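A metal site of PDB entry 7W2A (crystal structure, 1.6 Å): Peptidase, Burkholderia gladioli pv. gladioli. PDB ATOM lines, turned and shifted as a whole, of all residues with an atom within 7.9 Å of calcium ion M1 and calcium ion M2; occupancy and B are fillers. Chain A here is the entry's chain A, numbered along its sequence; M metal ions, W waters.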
ATOM      1  N   TYR A  59     -14.024   3.707   0.476  1.00  0.00           N
ATOM      2  CA  TYR A  59     -14.714   4.846  -0.089  1.00  0.00           C
ATOM      3  C   TYR A  59     -14.736   5.972   0.915  1.00  0.00           C
ATOM      4  O   TYR A  59     -14.642   5.755   2.134  1.00  0.00           O
ATOM      5  CB  TYR A  59     -16.143   4.508  -0.529  1.00  0.00           C
ATOM      6  CG  TYR A  59     -16.597   5.303  -1.726  1.00  0.00           C
ATOM      7  CD1 TYR A  59     -16.196   4.924  -2.997  1.00  0.00           C
ATOM      8  CD2 TYR A  59     -17.427   6.417  -1.594  1.00  0.00           C
ATOM      9  CE1 TYR A  59     -16.593   5.640  -4.114  1.00  0.00           C
ATOM     10  CE2 TYR A  59     -17.835   7.136  -2.702  1.00  0.00           C
ATOM     11  CZ  TYR A  59     -17.410   6.734  -3.948  1.00  0.00           C
ATOM     12  OH  TYR A  59     -17.826   7.437  -5.071  1.00  0.00           O
ATOM     13  N   ASP A  60     -14.869   7.190   0.393  1.00  0.00           N
ATOM     14  CA  ASP A  60     -14.837   8.419   1.180  1.00  0.00           C
ATOM     15  C   ASP A  60     -16.170   9.121   0.966  1.00  0.00           C
ATOM     16  O   ASP A  60     -16.419   9.675  -0.114  1.00  0.00           O
ATOM     17  CB  ASP A  60     -13.644   9.287   0.759  1.00  0.00           C
ATOM     18  CG  ASP A  60     -13.448  10.502   1.646  1.00  0.00           C
ATOM     19  OD1 ASP A  60     -14.411  10.982   2.296  1.00  0.00           O
ATOM     20  OD2 ASP A  60     -12.300  11.013   1.629  1.00  0.00           O
ATOM     21  N   PHE A  61     -17.031   9.069   1.985  1.00  0.00           N
ATOM     22  CA  PHE A  61     -18.370   9.631   1.879  1.00  0.00           C
ATOM     23  C   PHE A  61     -18.488  11.056   2.420  1.00  0.00           C
ATOM     24  O   PHE A  61     -19.599  11.570   2.539  1.00  0.00           O
ATOM     25  CB  PHE A  61     -19.365   8.705   2.581  1.00  0.00           C
ATOM     26  CG  PHE A  61     -19.707   7.500   1.768  1.00  0.00           C
ATOM     27  CD1 PHE A  61     -20.631   7.600   0.730  1.00  0.00           C
ATOM     28  CD2 PHE A  61     -19.063   6.294   1.983  1.00  0.00           C
ATOM     29  CE1 PHE A  61     -20.907   6.518  -0.057  1.00  0.00           C
ATOM     30  CE2 PHE A  61     -19.349   5.196   1.182  1.00  0.00           C
ATOM     31  CZ  PHE A  61     -20.273   5.316   0.168  1.00  0.00           C
ATOM     32  N   ILE A  62     -17.370  11.710   2.740  1.00  0.00           N
ATOM     33  CA  ILE A  62     -17.480  13.083   3.235  1.00  0.00           C
ATOM     34  C   ILE A  62     -17.881  13.996   2.085  1.00  0.00           C
ATOM     35  O   ILE A  62     -17.136  14.158   1.115  1.00  0.00           O
ATOM     36  CB  ILE A  62     -16.177  13.551   3.889  1.00  0.00           C
ATOM     37  CG1 ILE A  62     -15.787  12.625   5.053  1.00  0.00           C
ATOM     38  CG2 ILE A  62     -16.374  14.975   4.420  1.00  0.00           C
ATOM     39  CD1 ILE A  62     -14.438  13.018   5.688  1.00  0.00           C
ATOM     40  N   SER A  63     -19.067  14.587   2.190  1.00  0.00           N
ATOM     41  CA  SER A  63     -19.636  15.345   1.074  1.00  0.00           C
ATOM     42  C   SER A  63     -19.076  16.750   0.952  1.00  0.00           C
ATOM     43  O   SER A  63     -18.970  17.283  -0.162  1.00  0.00           O
ATOM     44  CB  SER A  63     -21.155  15.414   1.230  1.00  0.00           C
ATOM     45  OG  SER A  63     -21.724  14.120   1.173  1.00  0.00           O
ATOM     46  N   ASP A  64     -18.710  17.365   2.081  1.00  0.00           N
ATOM     47  CA  ASP A  64     -18.278  18.760   2.103  1.00  0.00           C
ATOM     48  C   ASP A  64     -16.774  18.825   1.892  1.00  0.00           C
ATOM     49  O   ASP A  64     -16.023  18.286   2.729  1.00  0.00           O
ATOM     50  CB  ASP A  64     -18.668  19.402   3.431  1.00  0.00           C
ATOM     51  CG  ASP A  64     -18.410  20.900   3.473  1.00  0.00           C
ATOM     52  OD1 ASP A  64     -17.773  21.467   2.561  1.00  0.00           O
ATOM     53  OD2 ASP A  64     -18.875  21.538   4.439  1.00  0.00           O
ATOM     54  N   PRO A  65     -16.286  19.470   0.833  1.00  0.00           N
ATOM     55  CA  PRO A  65     -14.826  19.507   0.627  1.00  0.00           C
ATOM     56  C   PRO A  65     -14.057  20.170   1.749  1.00  0.00           C
ATOM     57  O   PRO A  65     -12.903  19.788   1.976  1.00  0.00           O
ATOM     58  CB  PRO A  65     -14.678  20.282  -0.691  1.00  0.00           C
ATOM     59  CG  PRO A  65     -15.998  20.083  -1.398  1.00  0.00           C
ATOM     60  CD  PRO A  65     -17.030  20.045  -0.300  1.00  0.00           C
ATOM     61  N   SER A  67     -14.634  20.063   5.111  1.00  0.00           N
ATOM     62  CA  SER A  67     -14.409  19.012   6.106  1.00  0.00           C
ATOM     63  C   SER A  67     -13.563  17.885   5.552  1.00  0.00           C
ATOM     64  O   SER A  67     -12.709  17.325   6.260  1.00  0.00           O
ATOM     65  CB  SER A  67     -15.755  18.453   6.582  1.00  0.00           C
ATOM     66  OG  SER A  67     -15.541  17.410   7.509  1.00  0.00           O
ATOM     67  N   ALA A  68     -13.774  17.519   4.286  1.00  0.00           N
ATOM     68  CA  ALA A  68     -13.061  16.387   3.707  1.00  0.00           C
ATOM     69  C   ALA A  68     -11.559  16.635   3.644  1.00  0.00           C
ATOM     70  O   ALA A  68     -10.771  15.697   3.779  1.00  0.00           O
ATOM     71  CB  ALA A  68     -13.607  16.105   2.302  1.00  0.00           C
ATOM     72  N   ASN A  69     -11.144  17.888   3.418  1.00  0.00           N
ATOM     73  CA  ASN A  69      -9.720  18.257   3.528  1.00  0.00           C
ATOM     74  C   ASN A  69      -8.860  17.502   2.519  1.00  0.00           C
ATOM     75  O   ASN A  69      -7.676  17.252   2.763  1.00  0.00           O
ATOM     76  CB  ASN A  69      -9.223  18.044   4.961  1.00  0.00           C
ATOM     77  CG  ASN A  69      -7.961  18.823   5.263  1.00  0.00           C
ATOM     78  OD1 ASN A  69      -7.700  19.858   4.666  1.00  0.00           O
ATOM     79  ND2 ASN A  69      -7.189  18.341   6.221  1.00  0.00           N
ATOM     80  N   ASP A  70      -9.434  17.122   1.368  1.00  0.00           N
ATOM     81  CA  ASP A  70      -8.711  16.325   0.386  1.00  0.00           C
ATOM     82  C   ASP A  70      -8.950  16.825  -1.040  1.00  0.00           C
ATOM     83  O   ASP A  70      -8.583  16.123  -2.004  1.00  0.00           O
ATOM     84  CB  ASP A  70      -9.093  14.839   0.496  1.00  0.00           C
ATOM     85  CG  ASP A  70     -10.540  14.584   0.178  1.00  0.00           C
ATOM     86  OD1 ASP A  70     -11.282  15.559  -0.081  1.00  0.00           O
ATOM     87  OD2 ASP A  70     -10.967  13.401   0.193  1.00  0.00           O
ATOM     88  N   GLY A  71      -9.547  17.993  -1.201  1.00  0.00           N
ATOM     89  CA  GLY A  71      -9.695  18.605  -2.504  1.00  0.00           C
ATOM     90  C   GLY A  71     -10.996  18.313  -3.231  1.00  0.00           C
ATOM     91  O   GLY A  71     -11.156  18.772  -4.373  1.00  0.00           O
ATOM     92  N   ASN A  72     -11.918  17.573  -2.623  1.00  0.00           N
ATOM     93  CA  ASN A  72     -13.174  17.284  -3.302  1.00  0.00           C
ATOM     94  C   ASN A  72     -14.172  16.700  -2.304  1.00  0.00           C
ATOM     95  O   ASN A  72     -13.839  16.380  -1.153  1.00  0.00           O
ATOM     96  CB  ASN A  72     -12.952  16.320  -4.481  1.00  0.00           C
ATOM     97  CG  ASN A  72     -12.123  15.129  -4.112  1.00  0.00           C
ATOM     98  OD1 ASN A  72     -12.313  14.542  -3.058  1.00  0.00           O
ATOM     99  ND2 ASN A  72     -11.182  14.755  -4.975  1.00  0.00           N
ATOM    100  N   GLY A  73     -15.414  16.554  -2.772  1.00  0.00           N
ATOM    101  CA  GLY A  73     -16.451  15.875  -2.009  1.00  0.00           C
ATOM    102  C   GLY A  73     -16.275  14.360  -2.045  1.00  0.00           C
ATOM    103  O   GLY A  73     -15.152  13.866  -1.974  1.00  0.00           O
ATOM    104  N   ARG A  74     -17.363  13.618  -2.191  1.00  0.00           N
ATOM    105  CA  ARG A  74     -17.259  12.163  -2.090  1.00  0.00           C
ATOM    106  C   ARG A  74     -16.296  11.620  -3.149  1.00  0.00           C
ATOM    107  O   ARG A  74     -16.198  12.149  -4.259  1.00  0.00           O
ATOM    108  CB  ARG A  74     -18.629  11.528  -2.227  1.00  0.00           C
ATOM    109  CG  ARG A  74     -19.525  11.862  -1.041  1.00  0.00           C
ATOM    110  CD  ARG A  74     -20.749  10.941  -1.001  1.00  0.00           C
ATOM    111  NE  ARG A  74     -21.470  11.111   0.253  1.00  0.00           N
ATOM    112  CZ  ARG A  74     -22.682  10.627   0.493  1.00  0.00           C
ATOM    113  NH1 ARG A  74     -23.316   9.919  -0.443  1.00  0.00           N
ATOM    114  NH2 ARG A  74     -23.273  10.851   1.665  1.00  0.00           N
ATOM    115  N   ASP A  75     -15.545  10.584  -2.780  1.00  0.00           N
ATOM    116  CA  ASP A  75     -14.500  10.078  -3.666  1.00  0.00           C
ATOM    117  C   ASP A  75     -14.134   8.656  -3.245  1.00  0.00           C
ATOM    118  O   ASP A  75     -14.566   8.166  -2.190  1.00  0.00           O
ATOM    119  CB  ASP A  75     -13.271  11.011  -3.650  1.00  0.00           C
ATOM    120  CG  ASP A  75     -12.521  10.988  -2.322  1.00  0.00           C
ATOM    121  OD1 ASP A  75     -11.725  10.054  -2.136  1.00  0.00           O
ATOM    122  OD2 ASP A  75     -12.695  11.896  -1.491  1.00  0.00           O
ATOM    123  N   ASN A  76     -13.343   7.985  -4.079  1.00  0.00           N
ATOM    124  CA  ASN A  76     -13.040   6.576  -3.862  1.00  0.00           C
ATOM    125  C   ASN A  76     -11.736   6.332  -3.099  1.00  0.00           C
ATOM    126  O   ASN A  76     -11.248   5.198  -3.081  1.00  0.00           O
ATOM    127  CB  ASN A  76     -13.022   5.820  -5.200  1.00  0.00           C
ATOM    128  CG  ASN A  76     -11.865   6.210  -6.092  1.00  0.00           C
ATOM    129  OD1 ASN A  76     -11.042   7.065  -5.759  1.00  0.00           O
ATOM    130  ND2 ASN A  76     -11.786   5.555  -7.249  1.00  0.00           N
ATOM    131  N   ASN A  77     -11.202   7.349  -2.429  1.00  0.00           N
ATOM    132  CA  ASN A  77      -9.924   7.243  -1.712  1.00  0.00           C
ATOM    133  C   ASN A  77     -10.179   7.552  -0.235  1.00  0.00           C
ATOM    134  O   ASN A  77     -10.297   8.725   0.151  1.00  0.00           O
ATOM    135  CB  ASN A  77      -8.877   8.184  -2.309  1.00  0.00           C
ATOM    136  CG  ASN A  77      -7.521   8.062  -1.631  1.00  0.00           C
ATOM    137  OD1 ASN A  77      -7.362   7.322  -0.658  1.00  0.00           O
ATOM    138  ND2 ASN A  77      -6.534   8.781  -2.149  1.00  0.00           N
ATOM    139  N   ALA A  78     -10.214   6.494   0.587  1.00  0.00           N
ATOM    140  CA  ALA A  78     -10.482   6.619   2.020  1.00  0.00           C
ATOM    141  C   ALA A  78      -9.238   6.914   2.845  1.00  0.00           C
ATOM    142  O   ALA A  78      -9.281   6.814   4.077  1.00  0.00           O
ATOM    143  CB  ALA A  78     -11.174   5.342   2.534  1.00  0.00           C
ATOM    144  N   ALA A  79      -8.133   7.303   2.220  1.00  0.00           N
ATOM    145  CA  ALA A  79      -6.991   7.763   3.003  1.00  0.00           C
ATOM    146  C   ALA A  79      -7.349   8.995   3.839  1.00  0.00           C
ATOM    147  O   ALA A  79      -8.153   9.839   3.439  1.00  0.00           O
ATOM    148  CB  ALA A  79      -5.812   8.085   2.073  1.00  0.00           C
ATOM    149  N   ASP A  80      -6.743   9.069   5.027  1.00  0.00           N
ATOM    150  CA  ASP A  80      -7.009  10.155   5.963  1.00  0.00           C
ATOM    151  C   ASP A  80      -6.007  11.279   5.693  1.00  0.00           C
ATOM    152  O   ASP A  80      -4.802  11.092   5.926  1.00  0.00           O
ATOM    153  CB  ASP A  80      -6.877   9.656   7.402  1.00  0.00           C
ATOM    154  CG  ASP A  80      -7.331  10.663   8.451  1.00  0.00           C
ATOM    155  OD1 ASP A  80      -7.645  11.826   8.117  1.00  0.00           O
ATOM    156  OD2 ASP A  80      -7.365  10.293   9.661  1.00  0.00           O
ATOM    157  N   PRO A  81      -6.450  12.447   5.215  1.00  0.00           N
ATOM    158  CA  PRO A  81      -5.522  13.570   5.026  1.00  0.00           C
ATOM    159  C   PRO A  81      -5.198  14.292   6.308  1.00  0.00           C
ATOM    160  O   PRO A  81      -4.339  15.192   6.287  1.00  0.00           O
ATOM    161  CB  PRO A  81      -6.294  14.485   4.073  1.00  0.00           C
ATOM    162  CG  PRO A  81      -7.722  14.334   4.561  1.00  0.00           C
ATOM    163  CD  PRO A  81      -7.833  12.811   4.841  1.00  0.00           C
ATOM    164  N   ARG A 147     -14.488   6.268   4.916  1.00  0.00           N
ATOM    165  CA  ARG A 147     -14.149   7.543   5.539  1.00  0.00           C
ATOM    166  C   ARG A 147     -15.400   8.409   5.603  1.00  0.00           C
ATOM    167  O   ARG A 147     -16.003   8.718   4.580  1.00  0.00           O
ATOM    168  CB  ARG A 147     -13.018   8.233   4.778  1.00  0.00           C
ATOM    169  CG  ARG A 147     -12.697   9.635   5.303  1.00  0.00           C
ATOM    170  CD  ARG A 147     -11.351  10.141   4.813  1.00  0.00           C
ATOM    171  NE  ARG A 147     -11.036  11.381   5.530  1.00  0.00           N
ATOM    172  CZ  ARG A 147     -11.097  12.608   4.986  1.00  0.00           C
ATOM    173  NH1 ARG A 147     -11.381  12.760   3.700  1.00  0.00           N
ATOM    174  NH2 ARG A 147     -10.839  13.656   5.742  1.00  0.00           N
HETATM  175 CA    CA M   1     -13.070  14.073  -0.943  1.00  0.00          CA
HETATM  176 CA    CA M   2     -10.703  11.077  -0.132  1.00  0.00          CA
HETATM  177  O   HOH W   1      -9.134  11.683  -1.840  1.00  0.00           O
HETATM  178  O   HOH W   2     -14.450  13.389   0.894  1.00  0.00           O
HETATM  179  O   HOH W   3      -8.785  11.230   1.236  1.00  0.00           O
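The guanidinium group (NH2) of Arg 147 lies within hydrogen-bond range of the backbone carbonyl oxygen (O) of Ala 68, at 2.8 Å.
OD1 of Asp 60 sits at hydrogen-bond distance from N of Ile 62 (3.1 Å).
The side-chain carboxylate (OD1) of Asp 60 lies within salt-bridge range of the guanidinium group (NH1) of Arg 147, at 3.8 Å.
The guanidinium group of Arg 147 sits close to the side-chain carboxylate of Asp 70, 3.6 Å away.
OD1 of Asn 77 sits at hydrogen-bond distance from N of Ala 79, at 3.0 Å.
Merely in contact with calcium ion M1: Ala 68.
Five residues have an atom within 4 Å of calcium ion M1: Ala 68, Asp 70, Asn 72, Gly 73 and Asp 75.
Of the 23 residues printed, 4 come within 4 Å of calcium ion M2.
The nearest printed residue that does not touch calcium ion M2 is Arg 147 (4.2 Å).
Calcium ion M1 is bound by OD2 of Asp 75 (2.3 Å), OD1 of Asn 72 (2.3 Å), O of Gly 73 (2.3 Å), water W2 (2.4 Å), O of Asn 72 (2.4 Å), OD1 of Asp 70 (2.5 Å) and OD2 of Asp 70 (2.5 Å).
Calcium ion M2 is bound by water W3, at 2.4 Å.
Calcium ion M2 is bound by OD2 of Asp 70.
Calcium ion M2 is bound by OD2 of Asp 60, 2.4 Å away.
Calcium ion M2 is bound by water W1, 2.4 Å away.
The backbone carbonyl oxygen (O) of Asn 77 binds calcium ion M2, at 2.4 Å.
Calcium ion M2 is bound by OD1 of Asp 75 (2.5 Å).
OD2 of Asp 75 binds calcium ion M2, at 2.5 Å.
Water W2 bridges the side-chain carboxylate of Asp 60 (2.8 Å) and the backbone carbonyl oxygen of Ile 62 (2.8 Å).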
